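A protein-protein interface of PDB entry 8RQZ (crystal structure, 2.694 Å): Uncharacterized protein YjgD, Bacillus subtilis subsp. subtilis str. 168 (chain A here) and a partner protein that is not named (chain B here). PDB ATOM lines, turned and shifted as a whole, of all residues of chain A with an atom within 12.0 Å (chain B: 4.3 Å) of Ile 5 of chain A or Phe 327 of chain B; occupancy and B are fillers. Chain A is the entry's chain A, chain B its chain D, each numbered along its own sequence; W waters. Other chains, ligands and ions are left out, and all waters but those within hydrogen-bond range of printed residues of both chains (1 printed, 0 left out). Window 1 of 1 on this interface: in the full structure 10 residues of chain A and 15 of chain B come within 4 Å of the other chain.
The backbone carbonyl oxygen (O) of Arg 7 of chain A is in hydrogen-bond range of the backbone NH (N) of Phe 327 of chain B, at 2.7 Å.
O of Glu 688 of chain B lies close to O of Lys 3 of chain A, at 3.2 Å.
The guanidinium group (NH2) of Arg 7 of chain A is in hydrogen-bond range of a ring nitrogen (ND1) of His 326 of chain B, at 2.9 Å.
OE1 of Glu 329 of chain B lies within hydrogen-bond range of N of Ile 11 of chain A.
The side-chain amino group of Lys 6 of chain A lies within salt-bridge range of the side-chain carboxylate of Glu 688 of chain B, at 2.9 Å.
O of Glu 688 of chain B is in hydrogen-bond range of N of Ile 5 of chain A, 3.1 Å away.
The guanidinium group (NH2) of Arg 7 of chain A lies within salt-bridge range of the side-chain carboxylate (OD1) of Asp 325 of chain B.
The backbone carbonyl oxygen (O) of Lys 3 of chain A is in hydrogen-bond range of the guanidinium group (NH2) of Arg 322 of chain B (2.7 Å).
The backbone NH (N) of Gln 9 of chain A lies within hydrogen-bond range of the backbone carbonyl oxygen (O) of Phe 327 of chain B (2.8 Å).
N of Glu 329 of chain B lies within hydrogen-bond range of O of Gln 9 of chain A, 3.0 Å away.
The backbone carbonyl oxygen (O) of Ala 690 of chain B sits at hydrogen-bond distance from the guanidinium group (NH2) of Arg 322 of chain B (2.9 Å).
NH2 of Arg 322 of chain B lies within hydrogen-bond range of O of Glu 688 of chain B, at 2.9 Å.
OD1 of Asp 325 of chain B is in hydrogen-bond range of ND1 of His 326 of chain B (3.2 Å).
The guanidinium group of Arg 7 of chain A sits close to the side-chain amide nitrogen of Gln 9 of chain A.
The backbone carbonyl oxygen of Arg 328 of chain B lies within hydrogen-bond range of the backbone NH of Ile 321 of chain B (2.8 Å).
The backbone carbonyl oxygen of Leu 320 of chain B lies within hydrogen-bond range of the backbone NH of Val 693 of chain B, 2.8 Å away.
Arg 322 of chain B touches Ala 2 of chain A (CZ to CB, 3.5 Å).
O of Glu 688 of chain B touches CA of Ala 4 of chain A, at 3.5 Å.
Ile 5 of chain A touches Arg 322 of chain B.
Ile 5 of chain A touches Asp 325 of chain B (CG2 to O, 3.5 Å).
Ile 5 of chain A touches His 326 of chain B.
Phe 327 of chain B touches Ile 5 of chain A (CE2 to CG1, 3.6 Å).
Ile 8 of chain A touches Leu 320 of chain B.
Ile 8 of chain A touches Phe 327 of chain B.
Gln 9 of chain A touches His 326 of chain B (CG to CD2, 3.3 Å).
O of Gln 9 of chain A touches CA of Arg 328 of chain B, at 3.9 Å.
Ile 5 of chain A touches just these residues of chain B: Arg 322 (3.5 Å), Asp 325 (3.5 Å), His 326 (3.5 Å), Phe 327 (3.6 Å) and Glu 688 (3.1 Å).
Phe 327 of chain B touches four residues of chain A.
Arg 322 of chain B touches three residues of chain A.
Of the printed residues of chain A, Asp 325 of chain B touches Ile 5 and Arg 7.
Of chain A, only Ile 5, Arg 7 and Gln 9 come within 4 Å of His 326 of chain B.
Arg 328 of chain B touches just one residue of chain A: Gln 9.
Glu 329 of chain B touches just these residues of chain A: Gln 9, Lys 10 and Ile 11.
No residue of chain A comes within 4 Å of Ala 687 of chain B.
No residue of chain A comes within 4 Å of Val 693 of chain B.
Printed residues of chain B within 4 Å of Lys 6 of chain A: Glu 688.
Printed residues of chain B within 4 Å of Ile 11 of chain A: Glu 329.
Of the printed residues of chain B, Gln 9 of chain A touches His 326, Phe 327, Arg 328 and Glu 329.
Of the printed residues of chain B, Ala 2 of chain A touches Arg 322.
Printed residues of chain B within 4 Å of Ala 4 of chain A: Glu 688 (3.5 Å).
Leu 683 of chain B touches none of the printed residues of chain A.
Glu 12 of chain A touches none of the printed residues of chain B.
The nearest residue of chain B that does not touch Ile 5 of chain A is Leu 683 of chain B (4.2 Å).
Hydrophobic or aromatic side chains of chain A that line the printed part of chain B: Ala 2, Ala 4, Ile 5, Ile 8 and Ile 11.
Along chain A the printed residues that touch a printed residue of chain B span positions 2 to 11.
Printed residues of chain B that touch a printed residue of chain A: Leu 320, Arg 322, Asp 325, His 326, Phe 327, Arg 328, Glu 329 and Glu 688.
Hydrophobic or aromatic side chains of chain B that line the printed part of chain A: Leu 320, His 326 and Phe 327.
Along chain B the printed residues that touch a printed residue of chain A span positions 320 to 688.
Among the printed residues, 21 pairs touch across the chains.
Among the printed residues, Asp or Glu carboxylates within 4 Å of a Lys or Arg side-chain nitrogen of the other chain: Lys 6 of chain A with Glu 688 of chain B (2.9 Å) and Arg 7 of chain A with Asp 325 of chain B (3.0 Å).
Water W1 bridges NH2 of Arg 7 of chain A (2.9 Å) and OD1 of Asp 325 of chain B (3.1 Å).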
ATOM      1  N   ALA A   2      13.302 -10.367   6.785  1.00  0.00           N
ATOM      2  CA  ALA A   2      13.465  -9.673   5.508  1.00  0.00           C
ATOM      3  C   ALA A   2      14.627 -10.264   4.617  1.00  0.00           C
ATOM      4  O   ALA A   2      15.269 -11.222   5.039  1.00  0.00           O
ATOM      5  CB  ALA A   2      13.646  -8.178   5.776  1.00  0.00           C
ATOM      6  N   LYS A   3      14.847  -9.751   3.372  1.00  0.00           N
ATOM      7  CA  LYS A   3      15.901 -10.231   2.462  1.00  0.00           C
ATOM      8  C   LYS A   3      17.327  -9.929   2.978  1.00  0.00           C
ATOM      9  O   LYS A   3      17.515  -9.000   3.763  1.00  0.00           O
ATOM     10  CB  LYS A   3      15.713  -9.691   1.016  1.00  0.00           C
ATOM     11  CG  LYS A   3      16.185  -8.240   0.798  1.00  0.00           C
ATOM     12  CD  LYS A   3      16.585  -7.888  -0.663  1.00  0.00           C
ATOM     13  CE  LYS A   3      17.175  -6.491  -0.727  1.00  0.00           C
ATOM     14  NZ  LYS A   3      18.105  -6.301  -1.876  1.00  0.00           N
ATOM     15  N   ALA A   4      18.332 -10.683   2.501  1.00  0.00           N
ATOM     16  CA  ALA A   4      19.710 -10.475   2.939  1.00  0.00           C
ATOM     17  C   ALA A   4      20.322  -9.179   2.418  1.00  0.00           C
ATOM     18  O   ALA A   4      20.308  -8.925   1.217  1.00  0.00           O
ATOM     19  CB  ALA A   4      20.569 -11.655   2.526  1.00  0.00           C
ATOM     20  N   ILE A   5      20.870  -8.361   3.319  1.00  0.00           N
ATOM     21  CA  ILE A   5      21.571  -7.117   2.969  1.00  0.00           C
ATOM     22  C   ILE A   5      22.881  -7.028   3.772  1.00  0.00           C
ATOM     23  O   ILE A   5      22.948  -7.568   4.871  1.00  0.00           O
ATOM     24  CB  ILE A   5      20.694  -5.852   3.178  1.00  0.00           C
ATOM     25  CG1 ILE A   5      20.090  -5.824   4.577  1.00  0.00           C
ATOM     26  CG2 ILE A   5      19.616  -5.703   2.102  1.00  0.00           C
ATOM     27  CD1 ILE A   5      19.593  -4.511   4.960  1.00  0.00           C
ATOM     28  N   LYS A   6      23.918  -6.360   3.240  1.00  0.00           N
ATOM     29  CA  LYS A   6      25.179  -6.222   3.973  1.00  0.00           C
ATOM     30  C   LYS A   6      25.618  -4.769   4.146  1.00  0.00           C
ATOM     31  O   LYS A   6      26.298  -4.448   5.122  1.00  0.00           O
ATOM     32  CB  LYS A   6      26.296  -7.042   3.320  1.00  0.00           C
ATOM     33  CG  LYS A   6      26.112  -8.542   3.405  1.00  0.00           C
ATOM     34  CD  LYS A   6      27.217  -9.253   2.627  1.00  0.00           C
ATOM     35  CE  LYS A   6      27.064 -10.757   2.561  1.00  0.00           C
ATOM     36  NZ  LYS A   6      25.824 -11.203   1.853  1.00  0.00           N
ATOM     37  N   ARG A   7      25.245  -3.900   3.193  1.00  0.00           N
ATOM     38  CA  ARG A   7      25.644  -2.488   3.171  1.00  0.00           C
ATOM     39  C   ARG A   7      25.137  -1.708   4.368  1.00  0.00           C
ATOM     40  O   ARG A   7      23.954  -1.728   4.651  1.00  0.00           O
ATOM     41  CB  ARG A   7      25.178  -1.824   1.868  1.00  0.00           C
ATOM     42  CG  ARG A   7      26.040  -0.646   1.429  1.00  0.00           C
ATOM     43  CD  ARG A   7      25.604   0.003   0.139  1.00  0.00           C
ATOM     44  NE  ARG A   7      24.321   0.696   0.268  1.00  0.00           N
ATOM     45  CZ  ARG A   7      23.238   0.407  -0.453  1.00  0.00           C
ATOM     46  NH1 ARG A   7      23.280  -0.548  -1.378  1.00  0.00           N
ATOM     47  NH2 ARG A   7      22.122   1.109  -0.297  1.00  0.00           N
ATOM     48  N   ILE A   8      26.037  -1.033   5.083  1.00  0.00           N
ATOM     49  CA  ILE A   8      25.687  -0.242   6.260  1.00  0.00           C
ATOM     50  C   ILE A   8      26.009   1.235   6.009  1.00  0.00           C
ATOM     51  O   ILE A   8      27.154   1.563   5.699  1.00  0.00           O
ATOM     52  CB  ILE A   8      26.453  -0.771   7.504  1.00  0.00           C
ATOM     53  CG1 ILE A   8      26.026  -2.190   7.863  1.00  0.00           C
ATOM     54  CG2 ILE A   8      26.316   0.166   8.692  1.00  0.00           C
ATOM     55  CD1 ILE A   8      26.908  -2.850   8.906  1.00  0.00           C
ATOM     56  N   GLN A   9      25.007   2.125   6.129  1.00  0.00           N
ATOM     57  CA  GLN A   9      25.226   3.561   5.996  1.00  0.00           C
ATOM     58  C   GLN A   9      25.477   4.058   7.415  1.00  0.00           C
ATOM     59  O   GLN A   9      24.568   4.056   8.245  1.00  0.00           O
ATOM     60  CB  GLN A   9      24.020   4.286   5.366  1.00  0.00           C
ATOM     61  CG  GLN A   9      23.504   3.668   4.062  1.00  0.00           C
ATOM     62  CD  GLN A   9      24.286   3.985   2.796  1.00  0.00           C
ATOM     63  OE1 GLN A   9      25.210   4.821   2.778  1.00  0.00           O
ATOM     64  NE2 GLN A   9      23.924   3.318   1.697  1.00  0.00           N
ATOM     65  N   LYS A  10      26.733   4.418   7.705  1.00  0.00           N
ATOM     66  CA  LYS A  10      27.167   4.871   9.024  1.00  0.00           C
ATOM     67  C   LYS A  10      26.601   6.231   9.414  1.00  0.00           C
ATOM     68  O   LYS A  10      26.243   7.030   8.551  1.00  0.00           O
ATOM     69  CB  LYS A  10      28.702   4.875   9.118  1.00  0.00           C
ATOM     70  CG  LYS A  10      29.340   3.558   8.704  1.00  0.00           C
ATOM     71  CD  LYS A  10      30.423   3.116   9.675  1.00  0.00           C
ATOM     72  CE  LYS A  10      31.122   1.868   9.193  1.00  0.00           C
ATOM     73  NZ  LYS A  10      30.158   0.808   8.782  1.00  0.00           N
ATOM     74  N   ILE A  11      26.523   6.493  10.724  1.00  0.00           N
ATOM     75  CA  ILE A  11      25.999   7.755  11.223  1.00  0.00           C
ATOM     76  C   ILE A  11      27.085   8.843  11.111  1.00  0.00           C
ATOM     77  O   ILE A  11      28.268   8.583  11.343  1.00  0.00           O
ATOM     78  CB  ILE A  11      25.355   7.581  12.632  1.00  0.00           C
ATOM     79  CG1 ILE A  11      23.945   8.207  12.681  1.00  0.00           C
ATOM     80  CG2 ILE A  11      26.251   8.067  13.771  1.00  0.00           C
ATOM     81  CD1 ILE A  11      23.147   7.872  13.903  1.00  0.00           C
ATOM     82  N   GLU A  12      26.688  10.034  10.663  1.00  0.00           N
ATOM     83  CA  GLU A  12      27.624  11.124  10.433  1.00  0.00           C
ATOM     84  C   GLU A  12      28.162  11.792  11.691  1.00  0.00           C
ATOM     85  O   GLU A  12      27.481  12.609  12.315  1.00  0.00           O
ATOM     86  CB  GLU A  12      27.009  12.175   9.504  1.00  0.00           C
ATOM     87  CG  GLU A  12      27.996  13.244   9.068  1.00  0.00           C
ATOM     88  CD  GLU A  12      27.433  14.291   8.127  1.00  0.00           C
ATOM     89  OE1 GLU A  12      26.316  14.084   7.596  1.00  0.00           O
ATOM     90  OE2 GLU A  12      28.118  15.320   7.913  1.00  0.00           O
ATOM     91  N   LEU B 320      21.546  -1.208  14.145  1.00  0.00           N
ATOM     92  CA  LEU B 320      21.255  -1.053  12.724  1.00  0.00           C
ATOM     93  C   LEU B 320      19.780  -1.253  12.431  1.00  0.00           C
ATOM     94  O   LEU B 320      19.213  -2.287  12.775  1.00  0.00           O
ATOM     95  CB  LEU B 320      22.065  -2.063  11.912  1.00  0.00           C
ATOM     96  CG  LEU B 320      23.556  -1.960  12.060  1.00  0.00           C
ATOM     97  CD1 LEU B 320      24.231  -3.152  11.445  1.00  0.00           C
ATOM     98  CD2 LEU B 320      24.064  -0.668  11.462  1.00  0.00           C
ATOM     99  N   ILE B 321      19.163  -0.274  11.784  1.00  0.00           N
ATOM    100  CA  ILE B 321      17.773  -0.383  11.380  1.00  0.00           C
ATOM    101  C   ILE B 321      17.721  -0.425   9.855  1.00  0.00           C
ATOM    102  O   ILE B 321      18.212   0.492   9.206  1.00  0.00           O
ATOM    103  CB  ILE B 321      16.924   0.770  11.945  1.00  0.00           C
ATOM    104  CG1 ILE B 321      17.050   0.833  13.472  1.00  0.00           C
ATOM    105  CG2 ILE B 321      15.464   0.609  11.488  1.00  0.00           C
ATOM    106  CD1 ILE B 321      16.296   1.935  14.102  1.00  0.00           C
ATOM    107  N   ARG B 322      17.156  -1.486   9.286  1.00  0.00           N
ATOM    108  CA  ARG B 322      17.046  -1.635   7.840  1.00  0.00           C
ATOM    109  C   ARG B 322      16.327  -0.455   7.170  1.00  0.00           C
ATOM    110  O   ARG B 322      15.215  -0.103   7.558  1.00  0.00           O
ATOM    111  CB  ARG B 322      16.318  -2.945   7.515  1.00  0.00           C
ATOM    112  CG  ARG B 322      16.008  -3.168   6.042  1.00  0.00           C
ATOM    113  CD  ARG B 322      15.185  -4.417   5.852  1.00  0.00           C
ATOM    114  NE  ARG B 322      15.912  -5.605   6.291  1.00  0.00           N
ATOM    115  CZ  ARG B 322      16.605  -6.400   5.488  1.00  0.00           C
ATOM    116  NH1 ARG B 322      16.644  -6.167   4.182  1.00  0.00           N
ATOM    117  NH2 ARG B 322      17.229  -7.461   5.975  1.00  0.00           N
ATOM    118  N   ASP B 325      17.402  -1.262   0.867  1.00  0.00           N
ATOM    119  CA  ASP B 325      18.455  -2.189   0.437  1.00  0.00           C
ATOM    120  C   ASP B 325      19.755  -2.096   1.255  1.00  0.00           C
ATOM    121  O   ASP B 325      20.789  -2.616   0.824  1.00  0.00           O
ATOM    122  CB  ASP B 325      18.759  -1.995  -1.062  1.00  0.00           C
ATOM    123  CG  ASP B 325      19.360  -0.641  -1.424  1.00  0.00           C
ATOM    124  OD1 ASP B 325      19.208   0.318  -0.621  1.00  0.00           O
ATOM    125  OD2 ASP B 325      19.982  -0.535  -2.512  1.00  0.00           O
ATOM    126  N   HIS B 326      19.711  -1.425   2.413  1.00  0.00           N
ATOM    127  CA  HIS B 326      20.880  -1.251   3.267  1.00  0.00           C
ATOM    128  C   HIS B 326      20.483  -1.113   4.746  1.00  0.00           C
ATOM    129  O   HIS B 326      19.308  -1.000   5.073  1.00  0.00           O
ATOM    130  CB  HIS B 326      21.670  -0.015   2.818  1.00  0.00           C
ATOM    131  CG  HIS B 326      20.918   1.267   2.991  1.00  0.00           C
ATOM    132  ND1 HIS B 326      20.378   1.936   1.908  1.00  0.00           N
ATOM    133  CD2 HIS B 326      20.641   1.967   4.117  1.00  0.00           C
ATOM    134  CE1 HIS B 326      19.811   3.024   2.405  1.00  0.00           C
ATOM    135  NE2 HIS B 326      19.942   3.083   3.731  1.00  0.00           N
ATOM    136  N   PHE B 327      21.466  -1.125   5.638  1.00  0.00           N
ATOM    137  CA  PHE B 327      21.246  -0.950   7.061  1.00  0.00           C
ATOM    138  C   PHE B 327      21.621   0.460   7.421  1.00  0.00           C
ATOM    139  O   PHE B 327      22.651   0.955   6.985  1.00  0.00           O
ATOM    140  CB  PHE B 327      22.116  -1.914   7.866  1.00  0.00           C
ATOM    141  CG  PHE B 327      21.486  -3.266   8.040  1.00  0.00           C
ATOM    142  CD1 PHE B 327      20.228  -3.391   8.597  1.00  0.00           C
ATOM    143  CD2 PHE B 327      22.157  -4.413   7.662  1.00  0.00           C
ATOM    144  CE1 PHE B 327      19.651  -4.633   8.760  1.00  0.00           C
ATOM    145  CE2 PHE B 327      21.581  -5.657   7.833  1.00  0.00           C
ATOM    146  CZ  PHE B 327      20.327  -5.758   8.371  1.00  0.00           C
ATOM    147  N   ARG B 328      20.795   1.108   8.213  1.00  0.00           N
ATOM    148  CA  ARG B 328      21.055   2.462   8.655  1.00  0.00           C
ATOM    149  C   ARG B 328      21.567   2.393  10.088  1.00  0.00           C
ATOM    150  O   ARG B 328      20.951   1.721  10.914  1.00  0.00           O
ATOM    151  CB  ARG B 328      19.757   3.288   8.564  1.00  0.00           C
ATOM    152  CG  ARG B 328      19.695   4.526   9.463  1.00  0.00           C
ATOM    153  CD  ARG B 328      18.513   5.405   9.128  1.00  0.00           C
ATOM    154  NE  ARG B 328      17.245   4.675   9.157  1.00  0.00           N
ATOM    155  CZ  ARG B 328      16.476   4.552  10.231  1.00  0.00           C
ATOM    156  NH1 ARG B 328      16.842   5.099  11.384  1.00  0.00           N
ATOM    157  NH2 ARG B 328      15.337   3.882  10.162  1.00  0.00           N
ATOM    158  N   GLU B 329      22.671   3.092  10.399  1.00  0.00           N
ATOM    159  CA  GLU B 329      23.137   3.151  11.778  1.00  0.00           C
ATOM    160  C   GLU B 329      22.164   4.103  12.489  1.00  0.00           C
ATOM    161  O   GLU B 329      21.901   5.203  11.991  1.00  0.00           O
ATOM    162  CB  GLU B 329      24.577   3.666  11.860  1.00  0.00           C
ATOM    163  CG  GLU B 329      25.600   2.571  12.103  1.00  0.00           C
ATOM    164  CD  GLU B 329      27.028   3.055  12.259  1.00  0.00           C
ATOM    165  OE1 GLU B 329      27.233   4.274  12.452  1.00  0.00           O
ATOM    166  OE2 GLU B 329      27.949   2.211  12.181  1.00  0.00           O
ATOM    167  N   LEU B 683      27.846  -8.754  12.290  1.00  0.00           N
ATOM    168  CA  LEU B 683      26.724  -8.853  11.355  1.00  0.00           C
ATOM    169  C   LEU B 683      26.789 -10.239  10.745  1.00  0.00           C
ATOM    170  O   LEU B 683      27.296 -10.426   9.639  1.00  0.00           O
ATOM    171  CB  LEU B 683      26.760  -7.784  10.259  1.00  0.00           C
ATOM    172  CG  LEU B 683      25.475  -7.686   9.448  1.00  0.00           C
ATOM    173  CD1 LEU B 683      24.616  -6.561   9.939  1.00  0.00           C
ATOM    174  CD2 LEU B 683      25.775  -7.496   7.994  1.00  0.00           C
ATOM    175  N   ALA B 687      21.975 -12.039  10.712  1.00  0.00           N
ATOM    176  CA  ALA B 687      21.779 -10.601  10.886  1.00  0.00           C
ATOM    177  C   ALA B 687      21.514  -9.868   9.586  1.00  0.00           C
ATOM    178  O   ALA B 687      20.881  -8.821   9.618  1.00  0.00           O
ATOM    179  CB  ALA B 687      22.965  -9.984  11.604  1.00  0.00           C
ATOM    180  N   GLU B 688      21.966 -10.416   8.440  1.00  0.00           N
ATOM    181  CA  GLU B 688      21.707  -9.822   7.124  1.00  0.00           C
ATOM    182  C   GLU B 688      20.206  -9.838   6.802  1.00  0.00           C
ATOM    183  O   GLU B 688      19.717  -8.947   6.107  1.00  0.00           O
ATOM    184  CB  GLU B 688      22.470 -10.580   6.037  1.00  0.00           C
ATOM    185  CG  GLU B 688      23.970 -10.524   6.222  1.00  0.00           C
ATOM    186  CD  GLU B 688      24.759 -11.352   5.230  1.00  0.00           C
ATOM    187  OE1 GLU B 688      24.190 -11.747   4.188  1.00  0.00           O
ATOM    188  OE2 GLU B 688      25.957 -11.599   5.494  1.00  0.00           O
ATOM    189  N   ALA B 690      17.880  -9.520   9.107  1.00  0.00           N
ATOM    190  CA  ALA B 690      17.178  -8.789  10.149  1.00  0.00           C
ATOM    191  C   ALA B 690      16.669  -7.436   9.697  1.00  0.00           C
ATOM    192  O   ALA B 690      17.221  -6.827   8.792  1.00  0.00           O
ATOM    193  CB  ALA B 690      18.076  -8.622  11.367  1.00  0.00           C
ATOM    194  N   VAL B 693      19.219  -4.873  13.921  1.00  0.00           N
ATOM    195  CA  VAL B 693      20.354  -5.599  14.461  1.00  0.00           C
ATOM    196  C   VAL B 693      20.817  -4.835  15.686  1.00  0.00           C
ATOM    197  O   VAL B 693      21.058  -3.633  15.597  1.00  0.00           O
ATOM    198  CB  VAL B 693      21.505  -5.808  13.451  1.00  0.00           C
ATOM    199  CG1 VAL B 693      22.615  -6.656  14.062  1.00  0.00           C
ATOM    200  CG2 VAL B 693      20.994  -6.454  12.174  1.00  0.00           C
HETATM  201  O   HOH W   1      20.425   2.983  -1.739  1.00  0.00           O
